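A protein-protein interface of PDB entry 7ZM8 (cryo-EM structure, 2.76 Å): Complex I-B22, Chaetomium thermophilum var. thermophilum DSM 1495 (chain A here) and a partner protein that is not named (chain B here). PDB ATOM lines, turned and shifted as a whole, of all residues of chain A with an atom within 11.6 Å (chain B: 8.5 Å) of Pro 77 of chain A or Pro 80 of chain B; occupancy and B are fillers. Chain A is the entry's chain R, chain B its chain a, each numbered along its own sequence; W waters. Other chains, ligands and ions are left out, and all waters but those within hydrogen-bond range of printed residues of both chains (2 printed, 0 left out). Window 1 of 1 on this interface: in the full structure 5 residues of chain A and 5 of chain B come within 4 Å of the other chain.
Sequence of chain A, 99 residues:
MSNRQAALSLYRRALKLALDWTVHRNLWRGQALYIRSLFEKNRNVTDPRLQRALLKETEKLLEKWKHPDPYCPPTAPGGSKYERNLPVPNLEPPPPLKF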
ATOM      1  N   ARG A  12      -9.826 -11.153 -12.188  1.00  0.00           N
ATOM      2  CA  ARG A  12     -10.230 -12.429 -12.765  1.00  0.00           C
ATOM      3  C   ARG A  12      -9.443 -12.727 -14.033  1.00  0.00           C
ATOM      4  O   ARG A  12      -9.079 -13.880 -14.288  1.00  0.00           O
ATOM      5  CB  ARG A  12     -11.732 -12.444 -13.049  1.00  0.00           C
ATOM      6  CG  ARG A  12     -12.206 -13.796 -13.540  1.00  0.00           C
ATOM      7  CD  ARG A  12     -13.692 -13.872 -13.825  1.00  0.00           C
ATOM      8  NE  ARG A  12     -14.092 -13.047 -14.959  1.00  0.00           N
ATOM      9  CZ  ARG A  12     -15.355 -12.816 -15.303  1.00  0.00           C
ATOM     10  NH1 ARG A  12     -16.344 -13.364 -14.615  1.00  0.00           N
ATOM     11  NH2 ARG A  12     -15.628 -12.055 -16.352  1.00  0.00           N
ATOM     12  N   LYS A  16      -6.966 -16.022 -15.029  1.00  0.00           N
ATOM     13  CA  LYS A  16      -7.186 -16.911 -16.165  1.00  0.00           C
ATOM     14  C   LYS A  16      -5.935 -17.019 -17.028  1.00  0.00           C
ATOM     15  O   LYS A  16      -5.615 -18.099 -17.534  1.00  0.00           O
ATOM     16  CB  LYS A  16      -8.366 -16.425 -16.999  1.00  0.00           C
ATOM     17  CG  LYS A  16      -9.710 -16.643 -16.353  1.00  0.00           C
ATOM     18  CD  LYS A  16     -10.801 -16.786 -17.401  1.00  0.00           C
ATOM     19  CE  LYS A  16     -11.862 -17.779 -16.958  1.00  0.00           C
ATOM     20  NZ  LYS A  16     -11.323 -19.163 -16.874  1.00  0.00           N
ATOM     21  N   ASP A  69      -3.673 -18.912 -27.449  1.00  0.00           N
ATOM     22  CA  ASP A  69      -4.930 -19.655 -27.507  1.00  0.00           C
ATOM     23  C   ASP A  69      -5.483 -19.782 -26.099  1.00  0.00           C
ATOM     24  O   ASP A  69      -5.255 -20.782 -25.408  1.00  0.00           O
ATOM     25  CB  ASP A  69      -4.724 -21.032 -28.139  1.00  0.00           C
ATOM     26  CG  ASP A  69      -5.891 -21.455 -29.007  1.00  0.00           C
ATOM     27  OD1 ASP A  69      -6.941 -20.778 -28.971  1.00  0.00           O
ATOM     28  OD2 ASP A  69      -5.757 -22.464 -29.729  1.00  0.00           O
ATOM     29  N   PRO A  70      -6.208 -18.774 -25.628  1.00  0.00           N
ATOM     30  CA  PRO A  70      -6.795 -18.862 -24.293  1.00  0.00           C
ATOM     31  C   PRO A  70      -7.865 -19.936 -24.249  1.00  0.00           C
ATOM     32  O   PRO A  70      -8.540 -20.221 -25.241  1.00  0.00           O
ATOM     33  CB  PRO A  70      -7.397 -17.469 -24.073  1.00  0.00           C
ATOM     34  CG  PRO A  70      -6.859 -16.621 -25.175  1.00  0.00           C
ATOM     35  CD  PRO A  70      -6.604 -17.537 -26.311  1.00  0.00           C
ATOM     36  N   TYR A  71      -8.010 -20.546 -23.082  1.00  0.00           N
ATOM     37  CA  TYR A  71      -9.022 -21.572 -22.920  1.00  0.00           C
ATOM     38  C   TYR A  71     -10.418 -20.972 -23.010  1.00  0.00           C
ATOM     39  O   TYR A  71     -10.684 -19.888 -22.490  1.00  0.00           O
ATOM     40  CB  TYR A  71      -8.849 -22.282 -21.582  1.00  0.00           C
ATOM     41  CG  TYR A  71     -10.064 -23.073 -21.181  1.00  0.00           C
ATOM     42  CD1 TYR A  71     -10.375 -24.265 -21.815  1.00  0.00           C
ATOM     43  CD2 TYR A  71     -10.906 -22.627 -20.180  1.00  0.00           C
ATOM     44  CE1 TYR A  71     -11.487 -24.992 -21.461  1.00  0.00           C
ATOM     45  CE2 TYR A  71     -12.016 -23.347 -19.820  1.00  0.00           C
ATOM     46  CZ  TYR A  71     -12.302 -24.530 -20.461  1.00  0.00           C
ATOM     47  OH  TYR A  71     -13.412 -25.249 -20.100  1.00  0.00           O
ATOM     48  N   CYS A  72     -11.331 -21.656 -23.697  1.00  0.00           N
ATOM     49  CA  CYS A  72     -12.757 -21.241 -23.763  1.00  0.00           C
ATOM     50  C   CYS A  72     -13.593 -22.463 -23.387  1.00  0.00           C
ATOM     51  O   CYS A  72     -13.287 -23.552 -23.891  1.00  0.00           O
ATOM     52  CB  CYS A  72     -13.144 -20.787 -25.165  1.00  0.00           C
ATOM     53  SG  CYS A  72     -14.580 -19.689 -25.164  1.00  0.00           S
ATOM     54  N   PRO A  73     -14.589 -22.352 -22.487  1.00  0.00           N
ATOM     55  CA  PRO A  73     -15.456 -23.487 -22.181  1.00  0.00           C
ATOM     56  C   PRO A  73     -16.134 -23.906 -23.492  1.00  0.00           C
ATOM     57  O   PRO A  73     -16.410 -23.056 -24.297  1.00  0.00           O
ATOM     58  CB  PRO A  73     -16.424 -22.898 -21.149  1.00  0.00           C
ATOM     59  CG  PRO A  73     -15.667 -21.752 -20.532  1.00  0.00           C
ATOM     60  CD  PRO A  73     -14.870 -21.170 -21.677  1.00  0.00           C
ATOM     61  N   PRO A  74     -16.435 -25.200 -23.725  1.00  0.00           N
ATOM     62  CA  PRO A  74     -16.940 -25.658 -25.041  1.00  0.00           C
ATOM     63  C   PRO A  74     -18.217 -25.013 -25.585  1.00  0.00           C
ATOM     64  O   PRO A  74     -18.298 -24.854 -26.762  1.00  0.00           O
ATOM     65  CB  PRO A  74     -17.192 -27.150 -24.815  1.00  0.00           C
ATOM     66  CG  PRO A  74     -16.291 -27.515 -23.666  1.00  0.00           C
ATOM     67  CD  PRO A  74     -16.274 -26.294 -22.774  1.00  0.00           C
ATOM     68  N   THR A  75     -19.186 -24.705 -24.733  1.00  0.00           N
ATOM     69  CA  THR A  75     -20.485 -24.147 -25.168  1.00  0.00           C
ATOM     70  C   THR A  75     -20.459 -22.622 -25.149  1.00  0.00           C
ATOM     71  O   THR A  75     -21.469 -22.013 -25.516  1.00  0.00           O
ATOM     72  CB  THR A  75     -21.558 -24.712 -24.236  1.00  0.00           C
ATOM     73  OG1 THR A  75     -22.810 -24.086 -24.516  1.00  0.00           O
ATOM     74  CG2 THR A  75     -21.194 -24.544 -22.778  1.00  0.00           C
ATOM     75  N   ALA A  76     -19.362 -22.027 -24.717  1.00  0.00           N
ATOM     76  CA  ALA A  76     -19.212 -20.559 -24.656  1.00  0.00           C
ATOM     77  C   ALA A  76     -18.931 -19.979 -26.039  1.00  0.00           C
ATOM     78  O   ALA A  76     -18.515 -20.725 -26.919  1.00  0.00           O
ATOM     79  CB  ALA A  76     -18.080 -20.245 -23.720  1.00  0.00           C
ATOM     80  N   PRO A  77     -19.153 -18.672 -26.277  1.00  0.00           N
ATOM     81  CA  PRO A  77     -18.763 -18.080 -27.541  1.00  0.00           C
ATOM     82  C   PRO A  77     -17.262 -18.317 -27.683  1.00  0.00           C
ATOM     83  O   PRO A  77     -16.561 -18.080 -26.732  1.00  0.00           O
ATOM     84  CB  PRO A  77     -19.024 -16.601 -27.282  1.00  0.00           C
ATOM     85  CG  PRO A  77     -20.178 -16.592 -26.314  1.00  0.00           C
ATOM     86  CD  PRO A  77     -19.866 -17.747 -25.393  1.00  0.00           C
ATOM     87  N   GLY A  78     -16.797 -18.682 -28.875  1.00  0.00           N
ATOM     88  CA  GLY A  78     -15.374 -19.048 -29.016  1.00  0.00           C
ATOM     89  C   GLY A  78     -15.120 -20.503 -28.683  1.00  0.00           C
ATOM     90  O   GLY A  78     -13.954 -20.912 -28.743  1.00  0.00           O
ATOM     91  N   GLY A  79     -16.167 -21.249 -28.343  1.00  0.00           N
ATOM     92  CA  GLY A  79     -16.023 -22.652 -27.939  1.00  0.00           C
ATOM     93  C   GLY A  79     -16.337 -23.616 -29.068  1.00  0.00           C
ATOM     94  O   GLY A  79     -16.810 -23.160 -30.107  1.00  0.00           O
ATOM     95  N   SER A  80     -16.042 -24.896 -28.885  1.00  0.00           N
ATOM     96  CA  SER A  80     -16.204 -25.940 -29.926  1.00  0.00           C
ATOM     97  C   SER A  80     -17.655 -26.290 -30.281  1.00  0.00           C
ATOM     98  O   SER A  80     -17.886 -26.618 -31.445  1.00  0.00           O
ATOM     99  CB  SER A  80     -15.391 -27.128 -29.525  1.00  0.00           C
ATOM    100  OG  SER A  80     -14.012 -26.805 -29.517  1.00  0.00           O
ATOM    101  N   LYS A  81     -18.575 -26.266 -29.317  1.00  0.00           N
ATOM    102  CA  LYS A  81     -19.963 -26.723 -29.579  1.00  0.00           C
ATOM    103  C   LYS A  81     -20.866 -25.496 -29.631  1.00  0.00           C
ATOM    104  O   LYS A  81     -22.091 -25.647 -29.684  1.00  0.00           O
ATOM    105  CB  LYS A  81     -20.360 -27.663 -28.438  1.00  0.00           C
ATOM    106  CG  LYS A  81     -21.526 -28.598 -28.720  1.00  0.00           C
ATOM    107  CD  LYS A  81     -21.967 -29.375 -27.508  1.00  0.00           C
ATOM    108  CE  LYS A  81     -23.240 -30.158 -27.743  1.00  0.00           C
ATOM    109  NZ  LYS A  81     -23.058 -31.205 -28.777  1.00  0.00           N
ATOM    110  N   TYR A  82     -20.256 -24.319 -29.661  1.00  0.00           N
ATOM    111  CA  TYR A  82     -21.032 -23.061 -29.710  1.00  0.00           C
ATOM    112  C   TYR A  82     -21.815 -22.995 -31.022  1.00  0.00           C
ATOM    113  O   TYR A  82     -21.192 -23.182 -32.074  1.00  0.00           O
ATOM    114  CB  TYR A  82     -20.079 -21.878 -29.574  1.00  0.00           C
ATOM    115  CG  TYR A  82     -20.767 -20.543 -29.486  1.00  0.00           C
ATOM    116  CD1 TYR A  82     -21.724 -20.300 -28.517  1.00  0.00           C
ATOM    117  CD2 TYR A  82     -20.468 -19.529 -30.375  1.00  0.00           C
ATOM    118  CE1 TYR A  82     -22.365 -19.076 -28.429  1.00  0.00           C
ATOM    119  CE2 TYR A  82     -21.097 -18.301 -30.299  1.00  0.00           C
ATOM    120  CZ  TYR A  82     -22.047 -18.072 -29.324  1.00  0.00           C
ATOM    121  OH  TYR A  82     -22.667 -16.860 -29.250  1.00  0.00           O
ATOM    122  N   GLU A  83     -23.116 -22.703 -30.945  1.00  0.00           N
ATOM    123  CA  GLU A  83     -23.976 -22.565 -32.145  1.00  0.00           C
ATOM    124  C   GLU A  83     -24.071 -23.866 -32.946  1.00  0.00           C
ATOM    125  O   GLU A  83     -24.310 -23.763 -34.143  1.00  0.00           O
ATOM    126  CB  GLU A  83     -23.468 -21.400 -32.992  1.00  0.00           C
ATOM    127  CG  GLU A  83     -23.602 -20.066 -32.292  1.00  0.00           C
ATOM    128  CD  GLU A  83     -23.092 -18.884 -33.090  1.00  0.00           C
ATOM    129  OE1 GLU A  83     -22.424 -19.110 -34.115  1.00  0.00           O
ATOM    130  OE2 GLU A  83     -23.370 -17.741 -32.685  1.00  0.00           O
ATOM    131  N   ARG A  84     -23.956 -25.039 -32.314  1.00  0.00           N
ATOM    132  CA  ARG A  84     -23.905 -26.302 -33.089  1.00  0.00           C
ATOM    133  C   ARG A  84     -25.267 -26.718 -33.635  1.00  0.00           C
ATOM    134  O   ARG A  84     -25.364 -26.954 -34.867  1.00  0.00           O
ATOM    135  CB  ARG A  84     -23.249 -27.443 -32.314  1.00  0.00           C
ATOM    136  CG  ARG A  84     -23.552 -28.826 -32.864  1.00  0.00           C
ATOM    137  CD  ARG A  84     -22.689 -29.875 -32.206  1.00  0.00           C
ATOM    138  NE  ARG A  84     -21.290 -29.481 -32.263  1.00  0.00           N
ATOM    139  CZ  ARG A  84     -20.298 -30.177 -31.733  1.00  0.00           C
ATOM    140  NH1 ARG A  84     -20.546 -31.314 -31.113  1.00  0.00           N
ATOM    141  NH2 ARG A  84     -19.062 -29.734 -31.825  1.00  0.00           N
ATOM    142  N   LEU A  86     -28.251 -24.811 -33.432  1.00  0.00           N
ATOM    143  CA  LEU A  86     -29.046 -23.661 -32.964  1.00  0.00           C
ATOM    144  C   LEU A  86     -30.466 -23.839 -33.467  1.00  0.00           C
ATOM    145  O   LEU A  86     -30.631 -24.015 -34.686  1.00  0.00           O
ATOM    146  CB  LEU A  86     -28.424 -22.366 -33.475  1.00  0.00           C
ATOM    147  CG  LEU A  86     -27.420 -21.691 -32.552  1.00  0.00           C
ATOM    148  CD1 LEU A  86     -27.146 -20.277 -33.027  1.00  0.00           C
ATOM    149  CD2 LEU A  86     -27.925 -21.682 -31.122  1.00  0.00           C
ATOM    150  N   ARG B  75     -16.371  -7.010 -36.716  1.00  0.00           N
ATOM    151  CA  ARG B  75     -17.246  -7.261 -35.583  1.00  0.00           C
ATOM    152  C   ARG B  75     -16.764  -8.401 -34.705  1.00  0.00           C
ATOM    153  O   ARG B  75     -17.382  -8.660 -33.671  1.00  0.00           O
ATOM    154  CB  ARG B  75     -18.670  -7.514 -36.076  1.00  0.00           C
ATOM    155  CG  ARG B  75     -19.450  -6.228 -36.234  1.00  0.00           C
ATOM    156  CD  ARG B  75     -20.806  -6.435 -36.843  1.00  0.00           C
ATOM    157  NE  ARG B  75     -20.778  -6.173 -38.276  1.00  0.00           N
ATOM    158  CZ  ARG B  75     -21.299  -6.976 -39.194  1.00  0.00           C
ATOM    159  NH1 ARG B  75     -21.215  -6.657 -40.475  1.00  0.00           N
ATOM    160  NH2 ARG B  75     -21.909  -8.094 -38.831  1.00  0.00           N
ATOM    161  N   GLN B  76     -15.680  -9.080 -35.077  1.00  0.00           N
ATOM    162  CA  GLN B  76     -15.068 -10.057 -34.187  1.00  0.00           C
ATOM    163  C   GLN B  76     -14.378  -9.402 -33.001  1.00  0.00           C
ATOM    164  O   GLN B  76     -14.015 -10.104 -32.055  1.00  0.00           O
ATOM    165  CB  GLN B  76     -14.074 -10.924 -34.959  1.00  0.00           C
ATOM    166  CG  GLN B  76     -12.899 -10.168 -35.526  1.00  0.00           C
ATOM    167  CD  GLN B  76     -11.771 -11.082 -35.969  1.00  0.00           C
ATOM    168  OE1 GLN B  76     -11.880 -11.770 -36.980  1.00  0.00           O
ATOM    169  NE2 GLN B  76     -10.689 -11.101 -35.207  1.00  0.00           N
ATOM    170  N   PHE B  77     -14.192  -8.088 -33.031  1.00  0.00           N
ATOM    171  CA  PHE B  77     -13.663  -7.337 -31.903  1.00  0.00           C
ATOM    172  C   PHE B  77     -14.754  -6.735 -31.035  1.00  0.00           C
ATOM    173  O   PHE B  77     -14.440  -5.989 -30.103  1.00  0.00           O
ATOM    174  CB  PHE B  77     -12.736  -6.235 -32.398  1.00  0.00           C
ATOM    175  CG  PHE B  77     -11.600  -6.741 -33.227  1.00  0.00           C
ATOM    176  CD1 PHE B  77     -10.672  -7.606 -32.689  1.00  0.00           C
ATOM    177  CD2 PHE B  77     -11.468  -6.363 -34.547  1.00  0.00           C
ATOM    178  CE1 PHE B  77      -9.640  -8.072 -33.441  1.00  0.00           C
ATOM    179  CE2 PHE B  77     -10.433  -6.830 -35.305  1.00  0.00           C
ATOM    180  CZ  PHE B  77      -9.517  -7.685 -34.752  1.00  0.00           C
ATOM    181  N   ARG B  78     -16.017  -7.026 -31.321  1.00  0.00           N
ATOM    182  CA  ARG B  78     -17.099  -6.628 -30.443  1.00  0.00           C
ATOM    183  C   ARG B  78     -17.245  -7.632 -29.310  1.00  0.00           C
ATOM    184  O   ARG B  78     -16.702  -8.737 -29.346  1.00  0.00           O
ATOM    185  CB  ARG B  78     -18.409  -6.507 -31.217  1.00  0.00           C
ATOM    186  CG  ARG B  78     -18.382  -5.462 -32.300  1.00  0.00           C
ATOM    187  CD  ARG B  78     -19.775  -5.110 -32.737  1.00  0.00           C
ATOM    188  NE  ARG B  78     -19.763  -4.021 -33.699  1.00  0.00           N
ATOM    189  CZ  ARG B  78     -20.849  -3.398 -34.135  1.00  0.00           C
ATOM    190  NH1 ARG B  78     -20.739  -2.416 -35.012  1.00  0.00           N
ATOM    191  NH2 ARG B  78     -22.043  -3.753 -33.692  1.00  0.00           N
ATOM    192  N   ASP B  79     -17.985  -7.230 -28.288  1.00  0.00           N
ATOM    193  CA  ASP B  79     -18.213  -8.099 -27.144  1.00  0.00           C
ATOM    194  C   ASP B  79     -19.218  -9.177 -27.523  1.00  0.00           C
ATOM    195  O   ASP B  79     -20.328  -8.849 -27.949  1.00  0.00           O
ATOM    196  CB  ASP B  79     -18.722  -7.298 -25.957  1.00  0.00           C
ATOM    197  CG  ASP B  79     -18.462  -7.987 -24.634  1.00  0.00           C
ATOM    198  OD1 ASP B  79     -17.829  -9.061 -24.628  1.00  0.00           O
ATOM    199  OD2 ASP B  79     -18.887  -7.448 -23.592  1.00  0.00           O
ATOM    200  N   PRO B  80     -18.872 -10.462 -27.403  1.00  0.00           N
ATOM    201  CA  PRO B  80     -19.865 -11.513 -27.651  1.00  0.00           C
ATOM    202  C   PRO B  80     -20.922 -11.616 -26.573  1.00  0.00           C
ATOM    203  O   PRO B  80     -21.899 -12.350 -26.763  1.00  0.00           O
ATOM    204  CB  PRO B  80     -19.014 -12.784 -27.712  1.00  0.00           C
ATOM    205  CG  PRO B  80     -17.822 -12.466 -26.912  1.00  0.00           C
ATOM    206  CD  PRO B  80     -17.540 -11.017 -27.126  1.00  0.00           C
ATOM    207  N   HIS B  81     -20.765 -10.914 -25.453  1.00  0.00           N
ATOM    208  CA  HIS B  81     -21.691 -11.004 -24.335  1.00  0.00           C
ATOM    209  C   HIS B  81     -22.563  -9.770 -24.184  1.00  0.00           C
ATOM    210  O   HIS B  81     -23.293  -9.658 -23.195  1.00  0.00           O
ATOM    211  CB  HIS B  81     -20.923 -11.254 -23.045  1.00  0.00           C
ATOM    212  CG  HIS B  81     -20.045 -12.459 -23.103  1.00  0.00           C
ATOM    213  ND1 HIS B  81     -18.682 -12.372 -23.264  1.00  0.00           N
ATOM    214  CD2 HIS B  81     -20.336 -13.778 -23.032  1.00  0.00           C
ATOM    215  CE1 HIS B  81     -18.168 -13.587 -23.290  1.00  0.00           C
ATOM    216  NE2 HIS B  81     -19.151 -14.457 -23.150  1.00  0.00           N
ATOM    217  N   ALA B  82     -22.507  -8.841 -25.129  1.00  0.00           N
ATOM    218  CA  ALA B  82     -23.385  -7.692 -25.053  1.00  0.00           C
ATOM    219  C   ALA B  82     -24.797  -8.090 -25.469  1.00  0.00           C
ATOM    220  O   ALA B  82     -25.020  -9.136 -26.082  1.00  0.00           O
ATOM    221  CB  ALA B  82     -22.862  -6.557 -25.929  1.00  0.00           C
ATOM    222  N   ASP B  83     -25.763  -7.243 -25.122  1.00  0.00           N
ATOM    223  CA  ASP B  83     -27.168  -7.531 -25.403  1.00  0.00           C
ATOM    224  C   ASP B  83     -27.485  -7.279 -26.878  1.00  0.00           C
ATOM    225  O   ASP B  83     -28.339  -6.473 -27.240  1.00  0.00           O
ATOM    226  CB  ASP B  83     -28.071  -6.709 -24.493  1.00  0.00           C
ATOM    227  CG  ASP B  83     -28.318  -7.381 -23.158  1.00  0.00           C
ATOM    228  OD1 ASP B  83     -28.318  -8.629 -23.115  1.00  0.00           O
ATOM    229  OD2 ASP B  83     -28.513  -6.663 -22.155  1.00  0.00           O
ATOM    230  N   TRP B  84     -26.773  -8.003 -27.733  1.00  0.00           N
ATOM    231  CA  TRP B  84     -26.949  -7.845 -29.167  1.00  0.00           C
ATOM    232  C   TRP B  84     -28.320  -8.338 -29.594  1.00  0.00           C
ATOM    233  O   TRP B  84     -28.777  -9.400 -29.167  1.00  0.00           O
ATOM    234  CB  TRP B  84     -25.871  -8.610 -29.929  1.00  0.00           C
ATOM    235  CG  TRP B  84     -24.480  -8.210 -29.601  1.00  0.00           C
ATOM    236  CD1 TRP B  84     -23.499  -9.010 -29.112  1.00  0.00           C
ATOM    237  CD2 TRP B  84     -23.904  -6.909 -29.744  1.00  0.00           C
ATOM    238  NE1 TRP B  84     -22.344  -8.295 -28.945  1.00  0.00           N
ATOM    239  CE2 TRP B  84     -22.567  -6.999 -29.324  1.00  0.00           C
ATOM    240  CE3 TRP B  84     -24.389  -5.678 -30.188  1.00  0.00           C
ATOM    241  CZ2 TRP B  84     -21.710  -5.907 -29.333  1.00  0.00           C
ATOM    242  CZ3 TRP B  84     -23.539  -4.601 -30.198  1.00  0.00           C
ATOM    243  CH2 TRP B  84     -22.212  -4.721 -29.774  1.00  0.00           C
ATOM    244  N   ASP B  86     -28.958  -9.314 -32.833  1.00  0.00           N
ATOM    245  CA  ASP B  86     -28.427 -10.510 -33.536  1.00  0.00           C
ATOM    246  C   ASP B  86     -27.132 -10.894 -32.833  1.00  0.00           C
ATOM    247  O   ASP B  86     -26.118 -10.294 -33.146  1.00  0.00           O
ATOM    248  CB  ASP B  86     -28.112 -10.211 -35.000  1.00  0.00           C
ATOM    249  CG  ASP B  86     -28.034 -11.448 -35.872  1.00  0.00           C
ATOM    250  OD1 ASP B  86     -28.011 -12.561 -35.316  1.00  0.00           O
ATOM    251  OD2 ASP B  86     -28.009 -11.287 -37.104  1.00  0.00           O
ATOM    252  N   LYS B  87     -27.190 -11.854 -31.924  1.00  0.00           N
ATOM    253  CA  LYS B  87     -26.007 -12.268 -31.141  1.00  0.00           C
ATOM    254  C   LYS B  87     -24.976 -12.903 -32.052  1.00  0.00           C
ATOM    255  O   LYS B  87     -23.786 -12.737 -31.774  1.00  0.00           O
ATOM    256  CB  LYS B  87     -26.414 -13.257 -30.051  1.00  0.00           C
ATOM    257  CG  LYS B  87     -27.404 -12.731 -29.023  1.00  0.00           C
ATOM    258  CD  LYS B  87     -26.759 -11.925 -27.917  1.00  0.00           C
ATOM    259  CE  LYS B  87     -27.726 -11.601 -26.799  1.00  0.00           C
ATOM    260  NZ  LYS B  87     -27.032 -11.054 -25.610  1.00  0.00           N
ATOM    261  N   GLN B  88     -25.415 -13.655 -33.051  1.00  0.00           N
ATOM    262  CA  GLN B  88     -24.480 -14.392 -33.925  1.00  0.00           C
ATOM    263  C   GLN B  88     -23.612 -13.383 -34.655  1.00  0.00           C
ATOM    264  O   GLN B  88     -22.409 -13.627 -34.795  1.00  0.00           O
ATOM    265  CB  GLN B  88     -25.247 -15.219 -34.948  1.00  0.00           C
ATOM    266  CG  GLN B  88     -26.156 -16.263 -34.328  1.00  0.00           C
ATOM    267  CD  GLN B  88     -26.930 -16.999 -35.392  1.00  0.00           C
ATOM    268  OE1 GLN B  88     -28.047 -17.450 -35.170  1.00  0.00           O
ATOM    269  NE2 GLN B  88     -26.340 -17.103 -36.569  1.00  0.00           N
ATOM    270  N   GLU B  89     -24.214 -12.294 -35.099  1.00  0.00           N
ATOM    271  CA  GLU B  89     -23.447 -11.314 -35.886  1.00  0.00           C
ATOM    272  C   GLU B  89     -22.900 -10.230 -34.969  1.00  0.00           C
ATOM    273  O   GLU B  89     -22.042  -9.482 -35.451  1.00  0.00           O
ATOM    274  CB  GLU B  89     -24.305 -10.794 -37.031  1.00  0.00           C
ATOM    275  CG  GLU B  89     -24.503 -11.817 -38.132  1.00  0.00           C
ATOM    276  CD  GLU B  89     -25.378 -11.361 -39.288  1.00  0.00           C
ATOM    277  OE1 GLU B  89     -25.919 -10.239 -39.211  1.00  0.00           O
ATOM    278  OE2 GLU B  89     -25.518 -12.129 -40.262  1.00  0.00           O
ATOM    279  N   ARG B  90     -23.342 -10.177 -33.710  1.00  0.00           N
ATOM    280  CA  ARG B  90     -22.933  -9.100 -32.765  1.00  0.00           C
ATOM    281  C   ARG B  90     -23.383  -7.736 -33.287  1.00  0.00           C
ATOM    282  O   ARG B  90     -22.556  -6.833 -33.389  1.00  0.00           O
ATOM    283  CB  ARG B  90     -21.454  -9.217 -32.395  1.00  0.00           C
ATOM    284  CG  ARG B  90     -21.053 -10.601 -31.914  1.00  0.00           C
ATOM    285  CD  ARG B  90     -19.578 -10.639 -31.602  1.00  0.00           C
ATOM    286  NE  ARG B  90     -19.138 -12.002 -31.386  1.00  0.00           N
ATOM    287  CZ  ARG B  90     -17.869 -12.356 -31.278  1.00  0.00           C
ATOM    288  NH1 ARG B  90     -16.922 -11.441 -31.372  1.00  0.00           N
ATOM    289  NH2 ARG B  90     -17.552 -13.622 -31.083  1.00  0.00           N
ATOM    290  N   MET B 106     -19.160 -11.364 -38.961  1.00  0.00           N
ATOM    291  CA  MET B 106     -18.642 -12.589 -38.368  1.00  0.00           C
ATOM    292  C   MET B 106     -18.345 -13.644 -39.421  1.00  0.00           C
ATOM    293  O   MET B 106     -17.500 -14.516 -39.201  1.00  0.00           O
ATOM    294  CB  MET B 106     -19.631 -13.125 -37.334  1.00  0.00           C
ATOM    295  CG  MET B 106     -19.680 -12.303 -36.052  1.00  0.00           C
ATOM    296  SD  MET B 106     -18.144 -12.218 -35.111  1.00  0.00           S
ATOM    297  CE  MET B 106     -17.535 -13.894 -35.239  1.00  0.00           C
HETATM  298  O   HOH W   1     -21.495 -16.277 -34.359  1.00  0.00           O
HETATM  299  O   HOH W   2     -24.184 -18.669 -36.174  1.00  0.00           O
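The side-chain sulfur (SG) of Cys 72 of chain A is in hydrogen-bond range of the backbone carbonyl oxygen (O) of Pro 77 of chain A.
Among the printed residues, merely in contact across the chains: Pro 77 of chain A with Pro 80 of chain B (3.8 Å), Pro 77 of chain A with His 81 of chain B (3.95 Å), Glu 83 of chain A with Gln 88 of chain B (3.6 Å) and Leu 86 of chain A with Gln 88 of chain B (3.7 Å).
Pro 80 of chain B touches just one residue of chain A: Pro 77.
No residue of chain A comes within 4 Å of Asp 79 of chain B.
Of chain A, only Pro 77 comes within 4 Å of His 81 of chain B.
No residue of chain A comes within 4 Å of Lys 87 of chain B.
Of the printed residues of chain B, Glu 83 of chain A touches Gln 88 (3.6 Å).
Of the printed residues of chain A, Gln 88 of chain B touches Glu 83 and Leu 86.
Lys 81 of chain A touches none of the printed residues of chain B.
The nearest residue of chain B that does not touch Pro 77 of chain A is Arg 90 of chain B (5.0 Å).
Of the 19 printed residues of chain A, 3 touch a printed residue of chain B.
Of the 16 printed residues of chain B, 3 touch a printed residue of chain A.
Hydrophobic or aromatic side chains of chain B within 4 Å of the printed part of chain A: Pro 80 and His 81.
Among the printed residues, 4 pairs touch across the chains.
Among the printed residues, no Asp or Glu carboxylate lies within 4 Å of a Lys or Arg side-chain nitrogen of the other chain.
Water W2 lies within hydrogen-bond range of the side-chain amide nitrogen of Gln 88 of chain B (2.7 Å) and the side-chain carboxylate of Glu 83 of chain A (2.7 Å).
Water W1 bridges O of Gln 88 of chain B and OE2 of Glu 83 of chain A.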
